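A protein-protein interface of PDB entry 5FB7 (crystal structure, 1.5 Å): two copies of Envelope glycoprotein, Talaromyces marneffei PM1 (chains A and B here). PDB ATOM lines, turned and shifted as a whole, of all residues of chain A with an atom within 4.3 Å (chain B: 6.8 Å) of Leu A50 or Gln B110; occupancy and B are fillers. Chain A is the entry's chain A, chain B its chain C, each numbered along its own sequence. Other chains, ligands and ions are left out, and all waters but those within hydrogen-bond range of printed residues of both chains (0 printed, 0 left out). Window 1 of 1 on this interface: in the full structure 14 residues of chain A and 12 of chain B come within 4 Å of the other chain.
NE2 of Gln A54 is in hydrogen-bond range of OD1 of Asn B43 (2.6 Å). The backbone carbonyl oxygen (O) of Gln A54 is in hydrogen-bond range of the side-chain amide nitrogen (ND2) of Asn B106. The side-chain amide nitrogen of Asn B107 is in hydrogen-bond range of the side-chain amide oxygen of Gln A54 (3.0 Å). NE2 of Gln A54 lies within hydrogen-bond range of OE1 of Gln B110 (2.7 Å). The side-chain carboxylate of Asp A51 lies close to the side-chain amide nitrogen of Asn B43 (2.3 Å).
The side-chain amide nitrogen of Asn B107 lies within hydrogen-bond range of the side-chain amide oxygen of Asn B43. The guanidinium group (NH2) of Arg B109 lies within hydrogen-bond range of the side-chain amide oxygen (OD1) of Asn B106, 3.4 Å away. OD1 of Asn B107 lies within hydrogen-bond range of NE2 of Gln B111 (3.0 Å).
Lys B47 touches Ile A46. O of Lys A47 touches ND2 of Asn B43 (3.98 Å). Leu A50 touches Asn B43. CB of Leu A50 touches OE1 of Gln B110 (3.7 Å). Gln B110 touches Val A53.
Of chain B, only Asn B43 (3.9 Å) and Gln B110 (3.7 Å) come within 4 Å of Leu A50. Of the printed residues of chain A, Gln B110 touches Leu A50 (3.7 Å), Val A53 (3.6 Å) and Gln A54 (2.7 Å). Printed residues of chain A within 4 Å of Asn B43: Lys A47, Leu A50, Asp A51 and Gln A54. Printed residues of chain A within 4 Å of Lys B47: Ile A46. Of the printed residues of chain A, Asn B106 touches Gln A54 (3.2 Å). Of the printed residues of chain B, Gln A54 touches Asn B43, Asn B106, Asn B107 and Gln B110. The nearest residue of chain B that does not touch Leu A50 is Ile B46 (4.2 Å).
Of the 10 printed residues of chain A, 6 touch a printed residue of chain B. Of the 17 printed residues of chain B, 5 touch a printed residue of chain A. Among the printed residues, no Asp or Glu carboxylate lies within 4 Å of a Lys or Arg side-chain nitrogen of the other chain.
Ile A46 touches Lys B47, but with the chains exchanged Lys A47 does not touch Ile B46 (7.4 Å). Positions printed for both chains: 46, 47, 50 and 114.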
ATOM      1  N   ILE A  46      -3.845 -18.634  21.469  1.00  0.00           N
ATOM      2  CA  ILE A  46      -3.990 -19.911  20.726  1.00  0.00           C
ATOM      3  C   ILE A  46      -5.446 -20.157  20.357  1.00  0.00           C
ATOM      4  O   ILE A  46      -5.749 -20.581  19.227  1.00  0.00           O
ATOM      5  CB  ILE A  46      -3.450 -21.087  21.578  1.00  0.00           C
ATOM      6  CG1 ILE A  46      -1.941 -20.942  21.764  1.00  0.00           C
ATOM      7  CG2 ILE A  46      -3.799 -22.442  20.941  1.00  0.00           C
ATOM      8  CD1 ILE A  46      -1.364 -21.684  22.920  1.00  0.00           C
ATOM      9  N   LYS A  47      -6.394 -19.935  21.278  1.00  0.00           N
ATOM     10  CA  LYS A  47      -7.793 -20.164  20.975  1.00  0.00           C
ATOM     11  C   LYS A  47      -8.267 -19.264  19.837  1.00  0.00           C
ATOM     12  O   LYS A  47      -8.962 -19.707  18.934  1.00  0.00           O
ATOM     13  CB  LYS A  47      -8.637 -20.017  22.228  1.00  0.00           C
ATOM     14  CG  LYS A  47      -8.363 -21.137  23.210  1.00  0.00           C
ATOM     15  CD  LYS A  47      -9.159 -20.990  24.491  1.00  0.00           C
ATOM     16  CE  LYS A  47      -8.639 -19.852  25.353  1.00  0.00           C
ATOM     17  NZ  LYS A  47      -8.948 -20.012  26.802  1.00  0.00           N
ATOM     18  N   ALA A  48      -7.829 -17.997  19.849  1.00  0.00           N
ATOM     19  CA  ALA A  48      -8.182 -17.072  18.766  1.00  0.00           C
ATOM     20  C   ALA A  48      -7.652 -17.547  17.428  1.00  0.00           C
ATOM     21  O   ALA A  48      -8.298 -17.347  16.380  1.00  0.00           O
ATOM     22  CB  ALA A  48      -7.625 -15.665  19.062  1.00  0.00           C
ATOM     23  N   THR A  49      -6.449 -18.095  17.443  1.00  0.00           N
ATOM     24  CA  THR A  49      -5.789 -18.585  16.274  1.00  0.00           C
ATOM     25  C   THR A  49      -6.557 -19.791  15.706  1.00  0.00           C
ATOM     26  O   THR A  49      -6.911 -19.803  14.508  1.00  0.00           O
ATOM     27  CB  THR A  49      -4.341 -18.907  16.553  1.00  0.00           C
ATOM     28  OG1 THR A  49      -3.685 -17.726  17.080  1.00  0.00           O
ATOM     29  CG2 THR A  49      -3.626 -19.352  15.263  1.00  0.00           C
ATOM     30  N   LEU A  50      -6.925 -20.740  16.586  1.00  0.00           N
ATOM     31  CA  LEU A  50      -7.668 -21.877  16.146  1.00  0.00           C
ATOM     32  C   LEU A  50      -9.035 -21.490  15.695  1.00  0.00           C
ATOM     33  O   LEU A  50      -9.564 -22.091  14.735  1.00  0.00           O
ATOM     34  CB  LEU A  50      -7.713 -22.936  17.217  1.00  0.00           C
ATOM     35  CG  LEU A  50      -6.333 -23.523  17.538  1.00  0.00           C
ATOM     36  CD1 LEU A  50      -6.439 -24.510  18.646  1.00  0.00           C
ATOM     37  CD2 LEU A  50      -5.669 -24.090  16.275  1.00  0.00           C
ATOM     38  N   ASP A  51      -9.667 -20.555  16.406  1.00  0.00           N
ATOM     39  CA  ASP A  51     -11.011 -20.031  15.987  1.00  0.00           C
ATOM     40  C   ASP A  51     -10.900 -19.475  14.552  1.00  0.00           C
ATOM     41  O   ASP A  51     -11.777 -19.699  13.739  1.00  0.00           O
ATOM     42  CB  ASP A  51     -11.547 -18.919  16.922  1.00  0.00           C
ATOM     43  CG  ASP A  51     -12.072 -19.421  18.283  1.00  0.00           C
ATOM     44  OD1 ASP A  51     -12.341 -20.623  18.492  1.00  0.00           O
ATOM     45  OD2 ASP A  51     -12.221 -18.576  19.201  1.00  0.00           O
ATOM     46  N   GLY A  52      -9.798 -18.801  14.251  1.00  0.00           N
ATOM     47  CA  GLY A  52      -9.533 -18.330  12.887  1.00  0.00           C
ATOM     48  C   GLY A  52      -9.466 -19.418  11.831  1.00  0.00           C
ATOM     49  O   GLY A  52     -10.041 -19.274  10.729  1.00  0.00           O
ATOM     50  N   VAL A  53      -8.792 -20.520  12.124  1.00  0.00           N
ATOM     51  CA  VAL A  53      -8.707 -21.636  11.208  1.00  0.00           C
ATOM     52  C   VAL A  53     -10.120 -22.215  10.961  1.00  0.00           C
ATOM     53  O   VAL A  53     -10.554 -22.449   9.825  1.00  0.00           O
ATOM     54  CB  VAL A  53      -7.821 -22.745  11.770  1.00  0.00           C
ATOM     55  CG1 VAL A  53      -7.863 -23.980  10.884  1.00  0.00           C
ATOM     56  CG2 VAL A  53      -6.408 -22.228  11.913  1.00  0.00           C
ATOM     57  N   GLN A  54     -10.866 -22.386  12.020  1.00  0.00           N
ATOM     58  CA  GLN A  54     -12.156 -23.023  11.897  1.00  0.00           C
ATOM     59  C   GLN A  54     -13.114 -22.141  11.147  1.00  0.00           C
ATOM     60  O   GLN A  54     -14.023 -22.653  10.495  1.00  0.00           O
ATOM     61  CB  GLN A  54     -12.716 -23.339  13.241  1.00  0.00           C
ATOM     62  CG  GLN A  54     -11.961 -24.432  13.979  1.00  0.00           C
ATOM     63  CD  GLN A  54     -12.188 -24.404  15.452  1.00  0.00           C
ATOM     64  OE1 GLN A  54     -13.207 -23.890  15.942  1.00  0.00           O
ATOM     65  NE2 GLN A  54     -11.193 -24.846  16.201  1.00  0.00           N
ATOM     66  N   ALA A 114      -0.473 -23.869  15.996  1.00  0.00           N
ATOM     67  CA  ALA A 114      -1.722 -23.188  15.629  1.00  0.00           C
ATOM     68  C   ALA A 114      -1.463 -22.158  14.527  1.00  0.00           C
ATOM     69  O   ALA A 114      -2.240 -22.032  13.578  1.00  0.00           O
ATOM     70  CB  ALA A 114      -2.343 -22.538  16.836  1.00  0.00           C
ATOM     71  N   ASN B  43     -12.360 -25.147  21.634  1.00  0.00           N
ATOM     72  CA  ASN B  43     -10.967 -24.822  21.633  1.00  0.00           C
ATOM     73  C   ASN B  43     -10.270 -24.819  23.007  1.00  0.00           C
ATOM     74  O   ASN B  43      -9.116 -25.209  23.083  1.00  0.00           O
ATOM     75  CB  ASN B  43     -10.727 -23.552  20.820  1.00  0.00           C
ATOM     76  CG  ASN B  43     -11.084 -23.767  19.335  1.00  0.00           C
ATOM     77  OD1 ASN B  43     -10.705 -24.842  18.730  1.00  0.00           O
ATOM     78  ND2 ASN B  43     -11.527 -22.743  18.704  1.00  0.00           N
ATOM     79  N   ILE B  46      -9.545 -28.518  23.224  1.00  0.00           N
ATOM     80  CA  ILE B  46      -8.377 -28.864  22.461  1.00  0.00           C
ATOM     81  C   ILE B  46      -7.101 -28.463  23.228  1.00  0.00           C
ATOM     82  O   ILE B  46      -6.171 -29.229  23.310  1.00  0.00           O
ATOM     83  CB  ILE B  46      -8.417 -28.207  21.052  1.00  0.00           C
ATOM     84  CG1 ILE B  46      -9.533 -28.840  20.225  1.00  0.00           C
ATOM     85  CG2 ILE B  46      -7.071 -28.346  20.350  1.00  0.00           C
ATOM     86  CD1 ILE B  46     -10.021 -27.991  19.074  1.00  0.00           C
ATOM     87  N   LYS B  47      -7.113 -27.281  23.820  1.00  0.00           N
ATOM     88  CA  LYS B  47      -5.935 -26.862  24.610  1.00  0.00           C
ATOM     89  C   LYS B  47      -5.658 -27.762  25.784  1.00  0.00           C
ATOM     90  O   LYS B  47      -4.513 -28.140  26.020  1.00  0.00           O
ATOM     91  CB  LYS B  47      -6.106 -25.460  25.163  1.00  0.00           C
ATOM     92  CG  LYS B  47      -4.819 -25.005  25.919  1.00  0.00           C
ATOM     93  CD  LYS B  47      -3.864 -24.324  24.965  1.00  0.00           C
ATOM     94  CE  LYS B  47      -2.444 -24.066  25.460  1.00  0.00           C
ATOM     95  NZ  LYS B  47      -2.131 -24.180  26.885  1.00  0.00           N
ATOM     96  N   LEU B  50      -4.097 -30.988  24.343  1.00  0.00           N
ATOM     97  CA  LEU B  50      -2.677 -30.784  23.941  1.00  0.00           C
ATOM     98  C   LEU B  50      -1.751 -30.464  25.142  1.00  0.00           C
ATOM     99  O   LEU B  50      -0.607 -30.960  25.213  1.00  0.00           O
ATOM    100  CB  LEU B  50      -2.583 -29.694  22.961  1.00  0.00           C
ATOM    101  CG  LEU B  50      -3.297 -30.005  21.640  1.00  0.00           C
ATOM    102  CD1 LEU B  50      -3.117 -28.842  20.716  1.00  0.00           C
ATOM    103  CD2 LEU B  50      -2.803 -31.285  21.031  1.00  0.00           C
ATOM    104  N   GLU B 105     -17.911 -28.871  12.339  1.00  0.00           N
ATOM    105  CA  GLU B 105     -17.178 -29.935  11.678  1.00  0.00           C
ATOM    106  C   GLU B 105     -15.663 -29.718  11.885  1.00  0.00           C
ATOM    107  O   GLU B 105     -14.936 -30.640  12.178  1.00  0.00           O
ATOM    108  CB  GLU B 105     -17.548 -30.027  10.205  1.00  0.00           C
ATOM    109  CG  GLU B 105     -16.716 -30.972   9.378  1.00  0.00           C
ATOM    110  CD  GLU B 105     -17.101 -32.420   9.531  1.00  0.00           C
ATOM    111  OE1 GLU B 105     -16.528 -33.252   8.792  1.00  0.00           O
ATOM    112  OE2 GLU B 105     -17.976 -32.737  10.379  1.00  0.00           O
ATOM    113  N   ASN B 106     -15.222 -28.502  11.615  1.00  0.00           N
ATOM    114  CA  ASN B 106     -13.793 -28.185  11.616  1.00  0.00           C
ATOM    115  C   ASN B 106     -13.226 -28.269  13.023  1.00  0.00           C
ATOM    116  O   ASN B 106     -12.139 -28.790  13.217  1.00  0.00           O
ATOM    117  CB  ASN B 106     -13.601 -26.791  11.043  1.00  0.00           C
ATOM    118  CG  ASN B 106     -13.971 -26.714   9.570  1.00  0.00           C
ATOM    119  OD1 ASN B 106     -13.899 -27.712   8.863  1.00  0.00           O
ATOM    120  ND2 ASN B 106     -14.262 -25.520   9.090  1.00  0.00           N
ATOM    121  N   ASN B 107     -14.012 -27.875  14.015  1.00  0.00           N
ATOM    122  CA  ASN B 107     -13.605 -27.978  15.381  1.00  0.00           C
ATOM    123  C   ASN B 107     -13.470 -29.443  15.775  1.00  0.00           C
ATOM    124  O   ASN B 107     -12.488 -29.851  16.381  1.00  0.00           O
ATOM    125  CB  ASN B 107     -14.589 -27.233  16.241  1.00  0.00           C
ATOM    126  CG  ASN B 107     -14.160 -27.127  17.664  1.00  0.00           C
ATOM    127  OD1 ASN B 107     -14.279 -28.084  18.436  1.00  0.00           O
ATOM    128  ND2 ASN B 107     -13.791 -25.904  18.074  1.00  0.00           N
ATOM    129  N   LEU B 108     -14.466 -30.256  15.400  1.00  0.00           N
ATOM    130  CA  LEU B 108     -14.401 -31.693  15.653  1.00  0.00           C
ATOM    131  C   LEU B 108     -13.164 -32.377  14.977  1.00  0.00           C
ATOM    132  O   LEU B 108     -12.574 -33.293  15.558  1.00  0.00           O
ATOM    133  CB  LEU B 108     -15.693 -32.382  15.181  1.00  0.00           C
ATOM    134  CG  LEU B 108     -16.921 -32.077  16.049  1.00  0.00           C
ATOM    135  CD1 LEU B 108     -18.189 -32.573  15.344  1.00  0.00           C
ATOM    136  CD2 LEU B 108     -16.830 -32.698  17.430  1.00  0.00           C
ATOM    137  N   ARG B 109     -12.767 -31.939  13.787  1.00  0.00           N
ATOM    138  CA  ARG B 109     -11.608 -32.508  13.153  1.00  0.00           C
ATOM    139  C   ARG B 109     -10.352 -32.177  13.936  1.00  0.00           C
ATOM    140  O   ARG B 109      -9.472 -33.052  14.109  1.00  0.00           O
ATOM    141  CB  ARG B 109     -11.487 -32.047  11.725  1.00  0.00           C
ATOM    142  CG  ARG B 109     -12.492 -32.663  10.791  1.00  0.00           C
ATOM    143  CD  ARG B 109     -12.372 -32.052   9.400  1.00  0.00           C
ATOM    144  NE  ARG B 109     -13.336 -32.597   8.453  1.00  0.00           N
ATOM    145  CZ  ARG B 109     -13.835 -31.907   7.424  1.00  0.00           C
ATOM    146  NH1 ARG B 109     -14.749 -32.458   6.625  1.00  0.00           N
ATOM    147  NH2 ARG B 109     -13.421 -30.657   7.184  1.00  0.00           N
ATOM    148  N   GLN B 110     -10.309 -30.996  14.527  1.00  0.00           N
ATOM    149  CA  GLN B 110      -9.193 -30.618  15.402  1.00  0.00           C
ATOM    150  C   GLN B 110      -9.258 -31.397  16.733  1.00  0.00           C
ATOM    151  O   GLN B 110      -8.210 -31.798  17.281  1.00  0.00           O
ATOM    152  CB  GLN B 110      -9.161 -29.094  15.671  1.00  0.00           C
ATOM    153  CG  GLN B 110      -8.867 -28.230  14.472  1.00  0.00           C
ATOM    154  CD  GLN B 110      -8.617 -26.720  14.803  1.00  0.00           C
ATOM    155  OE1 GLN B 110      -8.891 -26.229  15.925  1.00  0.00           O
ATOM    156  NE2 GLN B 110      -8.222 -25.999  13.825  1.00  0.00           N
ATOM    157  N   GLN B 111     -10.454 -31.632  17.269  1.00  0.00           N
ATOM    158  CA  GLN B 111     -10.576 -32.474  18.465  1.00  0.00           C
ATOM    159  C   GLN B 111     -10.034 -33.879  18.192  1.00  0.00           C
ATOM    160  O   GLN B 111      -9.371 -34.452  19.032  1.00  0.00           O
ATOM    161  CB  GLN B 111     -12.066 -32.624  18.860  1.00  0.00           C
ATOM    162  CG  GLN B 111     -12.767 -31.327  19.149  1.00  0.00           C
ATOM    163  CD  GLN B 111     -12.455 -30.764  20.473  1.00  0.00           C
ATOM    164  OE1 GLN B 111     -11.734 -31.361  21.260  1.00  0.00           O
ATOM    165  NE2 GLN B 111     -12.872 -29.506  20.683  1.00  0.00           N
ATOM    166  N   GLU B 112     -10.365 -34.410  17.020  1.00  0.00           N
ATOM    167  CA  GLU B 112      -9.903 -35.758  16.628  1.00  0.00           C
ATOM    168  C   GLU B 112      -8.382 -35.828  16.572  1.00  0.00           C
ATOM    169  O   GLU B 112      -7.743 -36.798  17.035  1.00  0.00           O
ATOM    170  CB  GLU B 112     -10.489 -36.122  15.264  1.00  0.00           C
ATOM    171  CG  GLU B 112     -10.245 -37.560  14.841  1.00  0.00           C
ATOM    172  CD  GLU B 112     -10.811 -37.881  13.475  1.00  0.00           C
ATOM    173  OE1 GLU B 112     -10.616 -37.062  12.524  1.00  0.00           O
ATOM    174  OE2 GLU B 112     -11.581 -38.899  13.359  1.00  0.00           O
ATOM    175  N   GLU B 113      -7.775 -34.819  15.955  1.00  0.00           N
ATOM    176  CA  GLU B 113      -6.328 -34.777  15.837  1.00  0.00           C
ATOM    177  C   GLU B 113      -5.651 -34.710  17.214  1.00  0.00           C
ATOM    178  O   GLU B 113      -4.684 -35.453  17.488  1.00  0.00           O
ATOM    179  CB  GLU B 113      -5.881 -33.591  14.951  1.00  0.00           C
ATOM    180  CG  GLU B 113      -6.196 -33.801  13.470  1.00  0.00           C
ATOM    181  CD  GLU B 113      -5.817 -32.603  12.603  1.00  0.00           C
ATOM    182  OE1 GLU B 113      -6.462 -32.373  11.550  1.00  0.00           O
ATOM    183  OE2 GLU B 113      -4.861 -31.888  12.957  1.00  0.00           O
ATOM    184  N   ALA B 114      -6.188 -33.895  18.109  1.00  0.00           N
ATOM    185  CA  ALA B 114      -5.633 -33.741  19.438  1.00  0.00           C
ATOM    186  C   ALA B 114      -5.856 -34.977  20.285  1.00  0.00           C
ATOM    187  O   ALA B 114      -4.914 -35.469  20.967  1.00  0.00           O
ATOM    188  CB  ALA B 114      -6.224 -32.540  20.138  1.00  0.00           C
ATOM    189  N   ALA B 115      -7.051 -35.539  20.206  1.00  0.00           N
ATOM    190  CA  ALA B 115      -7.310 -36.802  20.901  1.00  0.00           C
ATOM    191  C   ALA B 115      -6.371 -37.897  20.415  1.00  0.00           C
ATOM    192  O   ALA B 115      -5.912 -38.731  21.225  1.00  0.00           O
ATOM    193  CB  ALA B 115      -8.758 -37.220  20.738  1.00  0.00           C
ATOM    194  N   GLN B 116      -6.086 -37.952  19.108  1.00  0.00           N
ATOM    195  CA  GLN B 116      -5.167 -38.994  18.598  1.00  0.00           C
ATOM    196  C   GLN B 116      -3.762 -38.824  19.176  1.00  0.00           C
ATOM    197  O   GLN B 116      -3.125 -39.790  19.593  1.00  0.00           O
ATOM    198  CB  GLN B 116      -5.128 -38.967  17.081  1.00  0.00           C
ATOM    199  CG  GLN B 116      -4.249 -39.942  16.387  1.00  0.00           C
ATOM    200  CD  GLN B 116      -4.229 -39.652  14.903  1.00  0.00           C
ATOM    201  OE1 GLN B 116      -5.128 -38.936  14.377  1.00  0.00           O
ATOM    202  NE2 GLN B 116      -3.176 -40.097  14.231  1.00  0.00           N
ATOM    203  N   ILE B 149     -18.090 -36.022  13.720  1.00  0.00           N
ATOM    204  CA  ILE B 149     -17.577 -35.561  12.430  1.00  0.00           C
ATOM    205  C   ILE B 149     -18.513 -35.930  11.306  1.00  0.00           C
ATOM    206  O   ILE B 149     -18.890 -35.063  10.491  1.00  0.00           O
ATOM    207  CB  ILE B 149     -16.155 -36.092  12.149  1.00  0.00           C
ATOM    208  CG1 ILE B 149     -15.179 -35.388  13.091  1.00  0.00           C
ATOM    209  CG2 ILE B 149     -15.781 -35.919  10.683  1.00  0.00           C
ATOM    210  CD1 ILE B 149     -13.789 -35.971  13.077  1.00  0.00           C
